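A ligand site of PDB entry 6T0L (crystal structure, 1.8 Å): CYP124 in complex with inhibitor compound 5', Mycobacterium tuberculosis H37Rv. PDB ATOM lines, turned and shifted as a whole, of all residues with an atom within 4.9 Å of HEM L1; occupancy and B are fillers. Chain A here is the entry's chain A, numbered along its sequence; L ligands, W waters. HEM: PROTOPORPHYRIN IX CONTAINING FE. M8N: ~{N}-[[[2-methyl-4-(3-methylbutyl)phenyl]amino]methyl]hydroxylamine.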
ATOM      1  N   MET A 117       0.132 -12.363  21.437  1.00  0.00           N
ATOM      2  CA  MET A 117       0.647 -12.427  20.074  1.00  0.00           C
ATOM      3  C   MET A 117       1.447 -13.706  19.792  1.00  0.00           C
ATOM      4  O   MET A 117       1.658 -14.061  18.620  1.00  0.00           O
ATOM      5  CB  MET A 117       1.521 -11.191  19.837  1.00  0.00           C
ATOM      6  CG  MET A 117       2.823 -11.272  20.578  1.00  0.00           C
ATOM      7  SD  MET A 117       3.690  -9.694  20.414  1.00  0.00           S
ATOM      8  CE  MET A 117       5.148 -10.014  21.403  1.00  0.00           C
ATOM      9  N   ILE A 118       1.881 -14.427  20.831  1.00  0.00           N
ATOM     10  CA  ILE A 118       2.687 -15.608  20.587  1.00  0.00           C
ATOM     11  C   ILE A 118       1.829 -16.773  20.103  1.00  0.00           C
ATOM     12  O   ILE A 118       2.376 -17.731  19.533  1.00  0.00           O
ATOM     13  CB  ILE A 118       3.517 -16.017  21.829  1.00  0.00           C
ATOM     14  CG1 ILE A 118       4.705 -16.871  21.401  1.00  0.00           C
ATOM     15  CG2 ILE A 118       2.645 -16.782  22.882  1.00  0.00           C
ATOM     16  CD1 ILE A 118       5.624 -17.332  22.541  1.00  0.00           C
ATOM     17  N   HIS A 125      -0.364 -10.634  14.631  1.00  0.00           N
ATOM     18  CA  HIS A 125       0.830 -10.774  15.468  1.00  0.00           C
ATOM     19  C   HIS A 125       1.789  -9.597  15.282  1.00  0.00           C
ATOM     20  O   HIS A 125       2.294  -9.046  16.270  1.00  0.00           O
ATOM     21  CB  HIS A 125       1.548 -12.087  15.170  1.00  0.00           C
ATOM     22  CG  HIS A 125       2.988 -12.072  15.574  1.00  0.00           C
ATOM     23  ND1 HIS A 125       3.995 -11.760  14.687  1.00  0.00           N
ATOM     24  CD2 HIS A 125       3.592 -12.322  16.765  1.00  0.00           C
ATOM     25  CE1 HIS A 125       5.160 -11.837  15.310  1.00  0.00           C
ATOM     26  NE2 HIS A 125       4.941 -12.161  16.573  1.00  0.00           N
ATOM     27  N   ARG A 129       3.027  -6.984  18.130  1.00  0.00           N
ATOM     28  CA  ARG A 129       4.445  -6.908  18.471  1.00  0.00           C
ATOM     29  C   ARG A 129       4.983  -5.495  18.282  1.00  0.00           C
ATOM     30  O   ARG A 129       5.805  -5.031  19.069  1.00  0.00           O
ATOM     31  CB  ARG A 129       5.249  -7.921  17.642  1.00  0.00           C
ATOM     32  CG  ARG A 129       6.805  -7.826  17.877  1.00  0.00           C
ATOM     33  CD  ARG A 129       7.539  -9.101  17.409  1.00  0.00           C
ATOM     34  NE  ARG A 129       8.991  -9.026  17.540  1.00  0.00           N
ATOM     35  CZ  ARG A 129       9.798 -10.047  17.841  1.00  0.00           C
ATOM     36  NH1 ARG A 129       9.296 -11.242  18.119  1.00  0.00           N
ATOM     37  NH2 ARG A 129      11.117  -9.875  17.916  1.00  0.00           N
ATOM     38  N   PHE A 136      12.743  -2.990  23.015  1.00  0.00           N
ATOM     39  CA  PHE A 136      13.686  -4.101  23.110  1.00  0.00           C
ATOM     40  C   PHE A 136      14.772  -4.014  22.038  1.00  0.00           C
ATOM     41  O   PHE A 136      15.547  -4.966  21.876  1.00  0.00           O
ATOM     42  CB  PHE A 136      12.917  -5.436  23.017  1.00  0.00           C
ATOM     43  CG  PHE A 136      12.061  -5.691  24.233  1.00  0.00           C
ATOM     44  CD1 PHE A 136      12.606  -6.264  25.367  1.00  0.00           C
ATOM     45  CD2 PHE A 136      10.728  -5.302  24.270  1.00  0.00           C
ATOM     46  CE1 PHE A 136      11.828  -6.458  26.520  1.00  0.00           C
ATOM     47  CE2 PHE A 136       9.956  -5.495  25.410  1.00  0.00           C
ATOM     48  CZ  PHE A 136      10.506  -6.079  26.539  1.00  0.00           C
ATOM     49  N   ILE A 183      12.560  -7.039  34.458  1.00  0.00           N
ATOM     50  CA  ILE A 183      11.318  -6.971  33.682  1.00  0.00           C
ATOM     51  C   ILE A 183      10.205  -6.270  34.488  1.00  0.00           C
ATOM     52  O   ILE A 183       9.397  -5.517  33.917  1.00  0.00           O
ATOM     53  CB  ILE A 183      10.893  -8.371  33.176  1.00  0.00           C
ATOM     54  CG1 ILE A 183       9.709  -8.272  32.202  1.00  0.00           C
ATOM     55  CG2 ILE A 183      10.468  -9.278  34.319  1.00  0.00           C
ATOM     56  CD1 ILE A 183      10.014  -7.535  30.927  1.00  0.00           C
ATOM     57  N   LEU A 270       2.274 -12.337  29.090  1.00  0.00           N
ATOM     58  CA  LEU A 270       3.333 -12.825  28.215  1.00  0.00           C
ATOM     59  C   LEU A 270       4.657 -12.157  28.540  1.00  0.00           C
ATOM     60  O   LEU A 270       5.678 -12.829  28.721  1.00  0.00           O
ATOM     61  CB  LEU A 270       2.988 -12.597  26.751  1.00  0.00           C
ATOM     62  CG  LEU A 270       4.155 -12.705  25.779  1.00  0.00           C
ATOM     63  CD1 LEU A 270       4.657 -14.189  25.624  1.00  0.00           C
ATOM     64  CD2 LEU A 270       3.738 -12.197  24.427  1.00  0.00           C
ATOM     65  N   LEU A 271       4.652 -10.826  28.643  1.00  0.00           N
ATOM     66  CA  LEU A 271       5.903 -10.092  28.860  1.00  0.00           C
ATOM     67  C   LEU A 271       6.529 -10.422  30.206  1.00  0.00           C
ATOM     68  O   LEU A 271       7.738 -10.635  30.299  1.00  0.00           O
ATOM     69  CB  LEU A 271       5.681  -8.582  28.740  1.00  0.00           C
ATOM     70  CG  LEU A 271       5.293  -8.137  27.336  1.00  0.00           C
ATOM     71  CD1 LEU A 271       4.673  -6.727  27.411  1.00  0.00           C
ATOM     72  CD2 LEU A 271       6.498  -8.146  26.393  1.00  0.00           C
ATOM     73  N   ALA A 274       7.681 -14.274  30.111  1.00  0.00           N
ATOM     74  CA  ALA A 274       8.807 -14.435  29.203  1.00  0.00           C
ATOM     75  C   ALA A 274      10.040 -13.701  29.723  1.00  0.00           C
ATOM     76  O   ALA A 274      11.163 -14.153  29.485  1.00  0.00           O
ATOM     77  CB  ALA A 274       8.464 -13.911  27.808  1.00  0.00           C
ATOM     78  N   GLY A 275       9.839 -12.587  30.443  1.00  0.00           N
ATOM     79  CA  GLY A 275      10.996 -11.801  30.829  1.00  0.00           C
ATOM     80  C   GLY A 275      11.771 -12.269  32.027  1.00  0.00           C
ATOM     81  O   GLY A 275      12.823 -11.697  32.316  1.00  0.00           O
ATOM     82  N   THR A 278      13.152 -17.756  31.746  1.00  0.00           N
ATOM     83  CA  THR A 278      14.174 -18.422  30.916  1.00  0.00           C
ATOM     84  C   THR A 278      15.567 -17.879  31.212  1.00  0.00           C
ATOM     85  O   THR A 278      16.555 -18.619  31.142  1.00  0.00           O
ATOM     86  CB  THR A 278      13.874 -18.248  29.432  1.00  0.00           C
ATOM     87  OG1 THR A 278      13.549 -16.874  29.196  1.00  0.00           O
ATOM     88  CG2 THR A 278      12.711 -19.107  28.993  1.00  0.00           C
ATOM     89  N   THR A 279      15.690 -16.562  31.444  1.00  0.00           N
ATOM     90  CA  THR A 279      16.999 -16.008  31.772  1.00  0.00           C
ATOM     91  C   THR A 279      17.506 -16.581  33.084  1.00  0.00           C
ATOM     92  O   THR A 279      18.719 -16.840  33.239  1.00  0.00           O
ATOM     93  CB  THR A 279      16.897 -14.479  31.848  1.00  0.00           C
ATOM     94  OG1 THR A 279      16.493 -13.988  30.564  1.00  0.00           O
ATOM     95  CG2 THR A 279      18.237 -13.874  32.193  1.00  0.00           C
ATOM     96  N   ALA A 282      18.972 -19.937  32.330  1.00  0.00           N
ATOM     97  CA  ALA A 282      20.231 -19.824  31.604  1.00  0.00           C
ATOM     98  C   ALA A 282      21.389 -19.534  32.552  1.00  0.00           C
ATOM     99  O   ALA A 282      22.465 -20.124  32.443  1.00  0.00           O
ATOM    100  CB  ALA A 282      20.133 -18.744  30.517  1.00  0.00           C
ATOM    101  N   VAL A 316      23.665 -20.384  26.271  1.00  0.00           N
ATOM    102  CA  VAL A 316      22.281 -20.542  25.848  1.00  0.00           C
ATOM    103  C   VAL A 316      22.110 -21.842  25.066  1.00  0.00           C
ATOM    104  O   VAL A 316      21.154 -22.589  25.295  1.00  0.00           O
ATOM    105  CB  VAL A 316      21.804 -19.336  25.029  1.00  0.00           C
ATOM    106  CG1 VAL A 316      20.392 -19.577  24.535  1.00  0.00           C
ATOM    107  CG2 VAL A 316      21.819 -18.086  25.948  1.00  0.00           C
ATOM    108  N   PRO A 321      17.003 -23.142  27.503  1.00  0.00           N
ATOM    109  CA  PRO A 321      15.979 -22.958  28.560  1.00  0.00           C
ATOM    110  C   PRO A 321      14.526 -23.264  28.137  1.00  0.00           C
ATOM    111  O   PRO A 321      13.729 -23.643  29.009  1.00  0.00           O
ATOM    112  CB  PRO A 321      16.156 -21.470  28.925  1.00  0.00           C
ATOM    113  CG  PRO A 321      17.588 -21.223  28.588  1.00  0.00           C
ATOM    114  CD  PRO A 321      17.778 -21.900  27.290  1.00  0.00           C
ATOM    115  N   VAL A 322      14.165 -23.038  26.877  1.00  0.00           N
ATOM    116  CA  VAL A 322      12.887 -23.470  26.311  1.00  0.00           C
ATOM    117  C   VAL A 322      13.160 -24.766  25.577  1.00  0.00           C
ATOM    118  O   VAL A 322      13.942 -24.781  24.611  1.00  0.00           O
ATOM    119  CB  VAL A 322      12.281 -22.420  25.356  1.00  0.00           C
ATOM    120  CG1 VAL A 322      10.921 -22.923  24.797  1.00  0.00           C
ATOM    121  CG2 VAL A 322      12.066 -21.111  26.086  1.00  0.00           C
ATOM    122  N   MET A 325       8.739 -25.479  21.387  1.00  0.00           N
ATOM    123  CA  MET A 325       7.497 -24.763  21.130  1.00  0.00           C
ATOM    124  C   MET A 325       6.680 -25.555  20.098  1.00  0.00           C
ATOM    125  O   MET A 325       7.234 -26.248  19.254  1.00  0.00           O
ATOM    126  CB  MET A 325       7.717 -23.358  20.585  1.00  0.00           C
ATOM    127  CG  MET A 325       8.291 -22.396  21.654  1.00  0.00           C
ATOM    128  SD  MET A 325       6.960 -21.608  22.550  1.00  0.00           S
ATOM    129  CE  MET A 325       7.939 -20.496  23.647  1.00  0.00           C
ATOM    130  N   ARG A 327       3.597 -25.979  17.048  1.00  0.00           N
ATOM    131  CA  ARG A 327       2.893 -25.375  15.911  1.00  0.00           C
ATOM    132  C   ARG A 327       1.721 -26.268  15.498  1.00  0.00           C
ATOM    133  O   ARG A 327       1.589 -27.389  15.979  1.00  0.00           O
ATOM    134  CB  ARG A 327       3.839 -25.154  14.720  1.00  0.00           C
ATOM    135  CG  ARG A 327       5.029 -24.192  15.027  1.00  0.00           C
ATOM    136  CD  ARG A 327       4.530 -22.796  15.188  1.00  0.00           C
ATOM    137  NE  ARG A 327       5.638 -21.828  15.217  1.00  0.00           N
ATOM    138  CZ  ARG A 327       6.226 -21.370  16.324  1.00  0.00           C
ATOM    139  NH1 ARG A 327       5.855 -21.823  17.512  1.00  0.00           N
ATOM    140  NH2 ARG A 327       7.208 -20.464  16.223  1.00  0.00           N
ATOM    141  N   TYR A 350      13.987 -27.588  20.428  1.00  0.00           N
ATOM    142  CA  TYR A 350      15.230 -26.817  20.416  1.00  0.00           C
ATOM    143  C   TYR A 350      16.333 -27.541  21.170  1.00  0.00           C
ATOM    144  O   TYR A 350      17.511 -27.431  20.811  1.00  0.00           O
ATOM    145  CB  TYR A 350      14.971 -25.444  21.060  1.00  0.00           C
ATOM    146  CG  TYR A 350      13.807 -24.674  20.451  1.00  0.00           C
ATOM    147  CD1 TYR A 350      13.732 -24.444  19.073  1.00  0.00           C
ATOM    148  CD2 TYR A 350      12.790 -24.188  21.268  1.00  0.00           C
ATOM    149  CE1 TYR A 350      12.667 -23.711  18.540  1.00  0.00           C
ATOM    150  CE2 TYR A 350      11.729 -23.445  20.737  1.00  0.00           C
ATOM    151  CZ  TYR A 350      11.684 -23.219  19.380  1.00  0.00           C
ATOM    152  OH  TYR A 350      10.608 -22.487  18.928  1.00  0.00           O
ATOM    153  N   GLY A 377      18.415 -21.595  20.660  1.00  0.00           N
ATOM    154  CA  GLY A 377      17.891 -21.354  22.003  1.00  0.00           C
ATOM    155  C   GLY A 377      16.808 -20.277  22.045  1.00  0.00           C
ATOM    156  O   GLY A 377      15.882 -20.355  22.855  1.00  0.00           O
ATOM    157  N   PHE A 378      16.920 -19.267  21.184  1.00  0.00           N
ATOM    158  CA  PHE A 378      15.888 -18.252  21.013  1.00  0.00           C
ATOM    159  C   PHE A 378      14.906 -18.626  19.924  1.00  0.00           C
ATOM    160  O   PHE A 378      14.180 -17.754  19.428  1.00  0.00           O
ATOM    161  CB  PHE A 378      16.545 -16.889  20.713  1.00  0.00           C
ATOM    162  CG  PHE A 378      17.425 -16.403  21.839  1.00  0.00           C
ATOM    163  CD1 PHE A 378      16.856 -16.004  23.059  1.00  0.00           C
ATOM    164  CD2 PHE A 378      18.795 -16.365  21.690  1.00  0.00           C
ATOM    165  CE1 PHE A 378      17.648 -15.553  24.127  1.00  0.00           C
ATOM    166  CE2 PHE A 378      19.630 -15.897  22.770  1.00  0.00           C
ATOM    167  CZ  PHE A 378      19.046 -15.515  23.990  1.00  0.00           C
ATOM    168  N   GLY A 379      14.830 -19.920  19.551  1.00  0.00           N
ATOM    169  CA  GLY A 379      13.947 -20.355  18.497  1.00  0.00           C
ATOM    170  C   GLY A 379      14.655 -20.481  17.181  1.00  0.00           C
ATOM    171  O   GLY A 379      15.852 -20.203  17.033  1.00  0.00           O
ATOM    172  N   GLY A 380      13.882 -20.919  16.177  1.00  0.00           N
ATOM    173  CA  GLY A 380      14.390 -21.135  14.836  1.00  0.00           C
ATOM    174  C   GLY A 380      14.494 -19.905  13.957  1.00  0.00           C
ATOM    175  O   GLY A 380      14.911 -20.042  12.803  1.00  0.00           O
ATOM    176  N   GLY A 381      14.161 -18.707  14.473  1.00  0.00           N
ATOM    177  CA  GLY A 381      14.226 -17.508  13.653  1.00  0.00           C
ATOM    178  C   GLY A 381      12.884 -17.202  13.029  1.00  0.00           C
ATOM    179  O   GLY A 381      11.894 -17.924  13.189  1.00  0.00           O
ATOM    180  N   ALA A 383       9.367 -15.007  12.332  1.00  0.00           N
ATOM    181  CA  ALA A 383       8.366 -14.034  12.766  1.00  0.00           C
ATOM    182  C   ALA A 383       8.284 -13.876  14.284  1.00  0.00           C
ATOM    183  O   ALA A 383       8.048 -12.773  14.793  1.00  0.00           O
ATOM    184  CB  ALA A 383       6.998 -14.450  12.214  1.00  0.00           C
ATOM    185  N   HIS A 384       8.460 -14.969  15.032  1.00  0.00           N
ATOM    186  CA  HIS A 384       8.326 -14.951  16.482  1.00  0.00           C
ATOM    187  C   HIS A 384       9.677 -14.949  17.210  1.00  0.00           C
ATOM    188  O   HIS A 384       9.708 -15.206  18.419  1.00  0.00           O
ATOM    189  CB  HIS A 384       7.464 -16.129  16.953  1.00  0.00           C
ATOM    190  CG  HIS A 384       6.031 -16.034  16.526  1.00  0.00           C
ATOM    191  ND1 HIS A 384       5.071 -15.371  17.268  1.00  0.00           N
ATOM    192  CD2 HIS A 384       5.374 -16.537  15.440  1.00  0.00           C
ATOM    193  CE1 HIS A 384       3.897 -15.467  16.672  1.00  0.00           C
ATOM    194  NE2 HIS A 384       4.056 -16.156  15.546  1.00  0.00           N
ATOM    195  N   PHE A 385      10.770 -14.635  16.502  1.00  0.00           N
ATOM    196  CA  PHE A 385      12.092 -14.656  17.123  1.00  0.00           C
ATOM    197  C   PHE A 385      12.065 -13.887  18.437  1.00  0.00           C
ATOM    198  O   PHE A 385      11.546 -12.764  18.498  1.00  0.00           O
ATOM    199  CB  PHE A 385      13.154 -14.066  16.203  1.00  0.00           C
ATOM    200  CG  PHE A 385      14.513 -14.006  16.836  1.00  0.00           C
ATOM    201  CD1 PHE A 385      15.282 -15.168  16.996  1.00  0.00           C
ATOM    202  CD2 PHE A 385      15.036 -12.788  17.285  1.00  0.00           C
ATOM    203  CE1 PHE A 385      16.516 -15.127  17.610  1.00  0.00           C
ATOM    204  CE2 PHE A 385      16.289 -12.733  17.908  1.00  0.00           C
ATOM    205  CZ  PHE A 385      17.030 -13.907  18.064  1.00  0.00           C
ATOM    206  N   CYS A 386      12.609 -14.495  19.484  1.00  0.00           N
ATOM    207  CA  CYS A 386      12.497 -13.988  20.856  1.00  0.00           C
ATOM    208  C   CYS A 386      12.637 -12.463  20.926  1.00  0.00           C
ATOM    209  O   CYS A 386      13.672 -11.905  20.545  1.00  0.00           O
ATOM    210  CB  CYS A 386      13.584 -14.624  21.730  1.00  0.00           C
ATOM    211  SG  CYS A 386      13.525 -13.944  23.446  1.00  0.00           S
ATOM    212  N   LEU A 387      11.612 -11.813  21.466  1.00  0.00           N
ATOM    213  CA  LEU A 387      11.649 -10.345  21.564  1.00  0.00           C
ATOM    214  C   LEU A 387      12.754  -9.878  22.519  1.00  0.00           C
ATOM    215  O   LEU A 387      13.317  -8.787  22.343  1.00  0.00           O
ATOM    216  CB  LEU A 387      10.288  -9.830  22.045  1.00  0.00           C
ATOM    217  CG  LEU A 387      10.082  -8.302  22.190  1.00  0.00           C
ATOM    218  CD1 LEU A 387      10.099  -7.617  20.843  1.00  0.00           C
ATOM    219  CD2 LEU A 387       8.813  -7.974  22.923  1.00  0.00           C
ATOM    220  N   GLY A 388      13.052 -10.662  23.562  1.00  0.00           N
ATOM    221  CA  GLY A 388      13.985 -10.214  24.570  1.00  0.00           C
ATOM    222  C   GLY A 388      15.413 -10.697  24.417  1.00  0.00           C
ATOM    223  O   GLY A 388      16.152 -10.671  25.394  1.00  0.00           O
ATOM    224  N   LEU A 391      18.270  -8.268  25.476  1.00  0.00           N
ATOM    225  CA  LEU A 391      18.213  -8.083  26.928  1.00  0.00           C
ATOM    226  C   LEU A 391      18.732  -9.310  27.672  1.00  0.00           C
ATOM    227  O   LEU A 391      19.491  -9.194  28.648  1.00  0.00           O
ATOM    228  CB  LEU A 391      16.777  -7.744  27.337  1.00  0.00           C
ATOM    229  CG  LEU A 391      16.524  -7.664  28.836  1.00  0.00           C
ATOM    230  CD1 LEU A 391      17.419  -6.515  29.445  1.00  0.00           C
ATOM    231  CD2 LEU A 391      15.069  -7.477  29.182  1.00  0.00           C
ATOM    232  N   ALA A 392      18.293 -10.508  27.255  1.00  0.00           N
ATOM    233  CA  ALA A 392      18.751 -11.721  27.924  1.00  0.00           C
ATOM    234  C   ALA A 392      20.255 -11.860  27.852  1.00  0.00           C
ATOM    235  O   ALA A 392      20.895 -12.211  28.845  1.00  0.00           O
ATOM    236  CB  ALA A 392      18.081 -12.951  27.290  1.00  0.00           C
ATOM    237  N   ILE A 396      22.734 -12.113  31.163  1.00  0.00           N
ATOM    238  CA  ILE A 396      23.661 -13.220  31.375  1.00  0.00           C
ATOM    239  C   ILE A 396      25.097 -12.724  31.510  1.00  0.00           C
ATOM    240  O   ILE A 396      25.811 -13.090  32.452  1.00  0.00           O
ATOM    241  CB  ILE A 396      23.532 -14.240  30.235  1.00  0.00           C
ATOM    242  CG1 ILE A 396      22.127 -14.825  30.228  1.00  0.00           C
ATOM    243  CG2 ILE A 396      24.590 -15.365  30.374  1.00  0.00           C
ATOM    244  CD1 ILE A 396      21.837 -15.577  28.917  1.00  0.00           C
HETATM  245  CHA HEM L   1       9.762 -15.794  22.271  1.00  0.00           C
HETATM  246  CHB HEM L   1      13.498 -18.126  24.237  1.00  0.00           C
HETATM  247  CHC HEM L   1      14.434 -14.305  27.108  1.00  0.00           C
HETATM  248  CHD HEM L   1      10.327 -12.225  25.522  1.00  0.00           C
HETATM  249  C1A HEM L   1      10.716 -16.738  22.534  1.00  0.00           C
HETATM  250  C2A HEM L   1      10.815 -18.049  21.898  1.00  0.00           C
HETATM  251  C3A HEM L   1      11.835 -18.674  22.446  1.00  0.00           C
HETATM  252  C4A HEM L   1      12.414 -17.821  23.458  1.00  0.00           C
HETATM  253  CMA HEM L   1      12.356 -20.086  22.108  1.00  0.00           C
HETATM  254  CAA HEM L   1       9.886 -18.551  20.773  1.00  0.00           C
HETATM  255  CBA HEM L   1      10.536 -18.192  19.428  1.00  0.00           C
HETATM  256  CGA HEM L   1       9.805 -18.756  18.228  1.00  0.00           C
HETATM  257  O1A HEM L   1      10.386 -18.685  17.104  1.00  0.00           O
HETATM  258  O2A HEM L   1       8.650 -19.223  18.402  1.00  0.00           O
HETATM  259  C1B HEM L   1      14.080 -17.293  25.186  1.00  0.00           C
HETATM  260  C2B HEM L   1      15.290 -17.600  25.921  1.00  0.00           C
HETATM  261  C3B HEM L   1      15.554 -16.537  26.720  1.00  0.00           C
HETATM  262  C4B HEM L   1      14.512 -15.543  26.513  1.00  0.00           C
HETATM  263  CMB HEM L   1      16.134 -18.912  25.845  1.00  0.00           C
HETATM  264  CAB HEM L   1      16.706 -16.362  27.723  1.00  0.00           C
HETATM  265  CBB HEM L   1      17.925 -16.931  27.703  1.00  0.00           C
HETATM  266  C1C HEM L   1      13.416 -13.418  26.915  1.00  0.00           C
HETATM  267  C2C HEM L   1      13.273 -12.169  27.613  1.00  0.00           C
HETATM  268  C3C HEM L   1      12.137 -11.588  27.212  1.00  0.00           C
HETATM  269  C4C HEM L   1      11.492 -12.466  26.216  1.00  0.00           C
HETATM  270  CMC HEM L   1      14.315 -11.608  28.629  1.00  0.00           C
HETATM  271  CAC HEM L   1      11.645 -10.183  27.703  1.00  0.00           C
HETATM  272  CBC HEM L   1      10.339  -9.947  27.816  1.00  0.00           C
HETATM  273  C1D HEM L   1       9.829 -13.020  24.511  1.00  0.00           C
HETATM  274  C2D HEM L   1       8.595 -12.764  23.801  1.00  0.00           C
HETATM  275  C3D HEM L   1       8.420 -13.771  22.890  1.00  0.00           C
HETATM  276  C4D HEM L   1       9.567 -14.655  23.018  1.00  0.00           C
HETATM  277  CMD HEM L   1       7.638 -11.577  24.054  1.00  0.00           C
HETATM  278  CAD HEM L   1       7.241 -13.902  21.877  1.00  0.00           C
HETATM  279  CBD HEM L   1       7.667 -13.190  20.586  1.00  0.00           C
HETATM  280  CGD HEM L   1       6.634 -13.244  19.480  1.00  0.00           C
HETATM  281  O1D HEM L   1       6.783 -12.488  18.484  1.00  0.00           O
HETATM  282  O2D HEM L   1       5.670 -14.052  19.594  1.00  0.00           O
HETATM  283  NA  HEM L   1      11.681 -16.665  23.492  1.00  0.00           N
HETATM  284  NB  HEM L   1      13.646 -16.022  25.550  1.00  0.00           N
HETATM  285  NC  HEM L   1      12.303 -13.554  26.087  1.00  0.00           N
HETATM  286  ND  HEM L   1      10.410 -14.178  24.033  1.00  0.00           N
HETATM  287 FE   HEM L   1      12.053 -15.101  24.838  1.00  0.00          FE
HETATM  288  C1  M8N L   2       5.313 -18.814  26.925  1.00  0.00           C
HETATM  289  C10 M8N L   2       3.200 -19.268  28.257  1.00  0.00           C
HETATM  290  C11 M8N L   2       2.498 -17.962  28.624  1.00  0.00           C
HETATM  291  C12 M8N L   2       2.754 -16.855  27.622  1.00  0.00           C
HETATM  292  C13 M8N L   2       2.854 -17.508  30.029  1.00  0.00           C
HETATM  293  C2  M8N L   2       5.745 -17.753  26.135  1.00  0.00           C
HETATM  294  C3  M8N L   2       7.053 -17.304  26.178  1.00  0.00           C
HETATM  295  C4  M8N L   2       7.974 -17.927  26.992  1.00  0.00           C
HETATM  296  C5  M8N L   2       7.592 -19.017  27.789  1.00  0.00           C
HETATM  297  C6  M8N L   2       6.257 -19.435  27.742  1.00  0.00           C
HETATM  298  C7  M8N L   2       8.585 -19.718  28.664  1.00  0.00           C
HETATM  299  C8  M8N L   2       9.909 -16.749  26.032  1.00  0.00           C
HETATM  300  C9  M8N L   2       3.875 -19.266  26.892  1.00  0.00           C
HETATM  301  N1  M8N L   2       9.342 -17.502  27.007  1.00  0.00           N
HETATM  302  N2  M8N L   2      10.926 -15.975  26.275  1.00  0.00           N
HETATM  303  O1  M8N L   2      11.324 -16.125  27.634  1.00  0.00           O
HETATM  304  O   HOH W   1      10.984 -21.318  16.583  1.00  0.00           O
HETATM  305  O   HOH W   2       9.746 -17.657  14.568  1.00  0.00           O
HETATM  306  O   HOH W   3       6.414 -19.939  19.805  1.00  0.00           O
HETATM  307  O   HOH W   4      12.982 -17.879  16.772  1.00  0.00           O
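The side-chain sulfur (SG) of Cys 386 binds an iron atom (FE) of HEM L1 (2.3 Å). O1D of HEM L1 lies within hydrogen-bond range of NE2 of His 125, 2.7 Å away. O2D of HEM L1 lies within hydrogen-bond range of ND1 of His 384. An oxygen (O1D) of HEM L1 lies within salt-bridge range of the guanidinium group of Arg 129, 2.8 Å away. The guanidinium group (NH2) of Arg 327 lies within salt-bridge range of an oxygen (O2A) of HEM L1 (2.9 Å). OG1 of Thr 278 lies within hydrogen-bond range of O1 of M8N L2 (2.8 Å). The backbone carbonyl oxygen (O) of Ala 274 is in hydrogen-bond range of an oxygen (O1) of M8N L2 (2.7 Å).
N2 of M8N L2 binds FE of HEM L1, at 2.0 Å.
The backbone NH of Gly 388 sits close to the side-chain sulfur of Cys 386. A ring nitrogen (NE2) of His 125 is in hydrogen-bond range of a ring nitrogen (ND1) of His 384. SD of Met 117 lies close to N of Arg 129, at 3.6 Å. The guanidinium group (NH1) of Arg 129 is in hydrogen-bond range of the backbone carbonyl oxygen (O) of Phe 385, at 2.7 Å.
Merely in contact with HEM L1: Met 117 (3.96 Å), Ile 118 (3.5 Å), Phe 136 (3.9 Å), Ile 183 (3.9 Å), Leu 270 (3.97 Å), Leu 271 (3.7 Å), Ala 274 (3.4 Å), Gly 275 (3.6 Å), Thr 278 (3.1 Å), Thr 279 (3.7 Å), Pro 321 (3.7 Å), Val 322 (3.8 Å), Met 325 (3.98 Å), Tyr 350 (3.7 Å), Gly 377 (3.3 Å), Phe 378 (3.5 Å), Gly 379 (3.6 Å), Ala 383 (3.9 Å), Leu 387 (3.7 Å), Gly 388 (3.5 Å) and Ala 392 (3.7 Å). Of the 33 residues printed, 26 come within 4 Å of HEM L1. Along chain A the residues within 4 Å of HEM L1 span positions 117 to 392.
Water W3 lies within hydrogen-bond range of an oxygen (O2A) of HEM L1, the guanidinium group (NH1) of Arg 327 and the side-chain sulfur (SD) of Met 325. Water W4 lies within hydrogen-bond range of the backbone NH of Gly 381 (2.7 Å), an oxygen (O1A) of HEM L1 (2.7 Å), the backbone carbonyl oxygen of Phe 378 (2.9 Å) and the backbone NH of Gly 380 (3.2 Å). Water W1 lies within hydrogen-bond range of OH of Tyr 350 (2.6 Å), O1A of HEM L1 (2.7 Å) and N of Gly 380 (3.0 Å). Water W2 lies within hydrogen-bond range of the backbone carbonyl oxygen of Gly 381 (2.6 Å), an oxygen (O1A) of HEM L1 (2.8 Å), the backbone NH of His 384 (3.0 Å) and the backbone NH of Ala 383 (3.5 Å).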
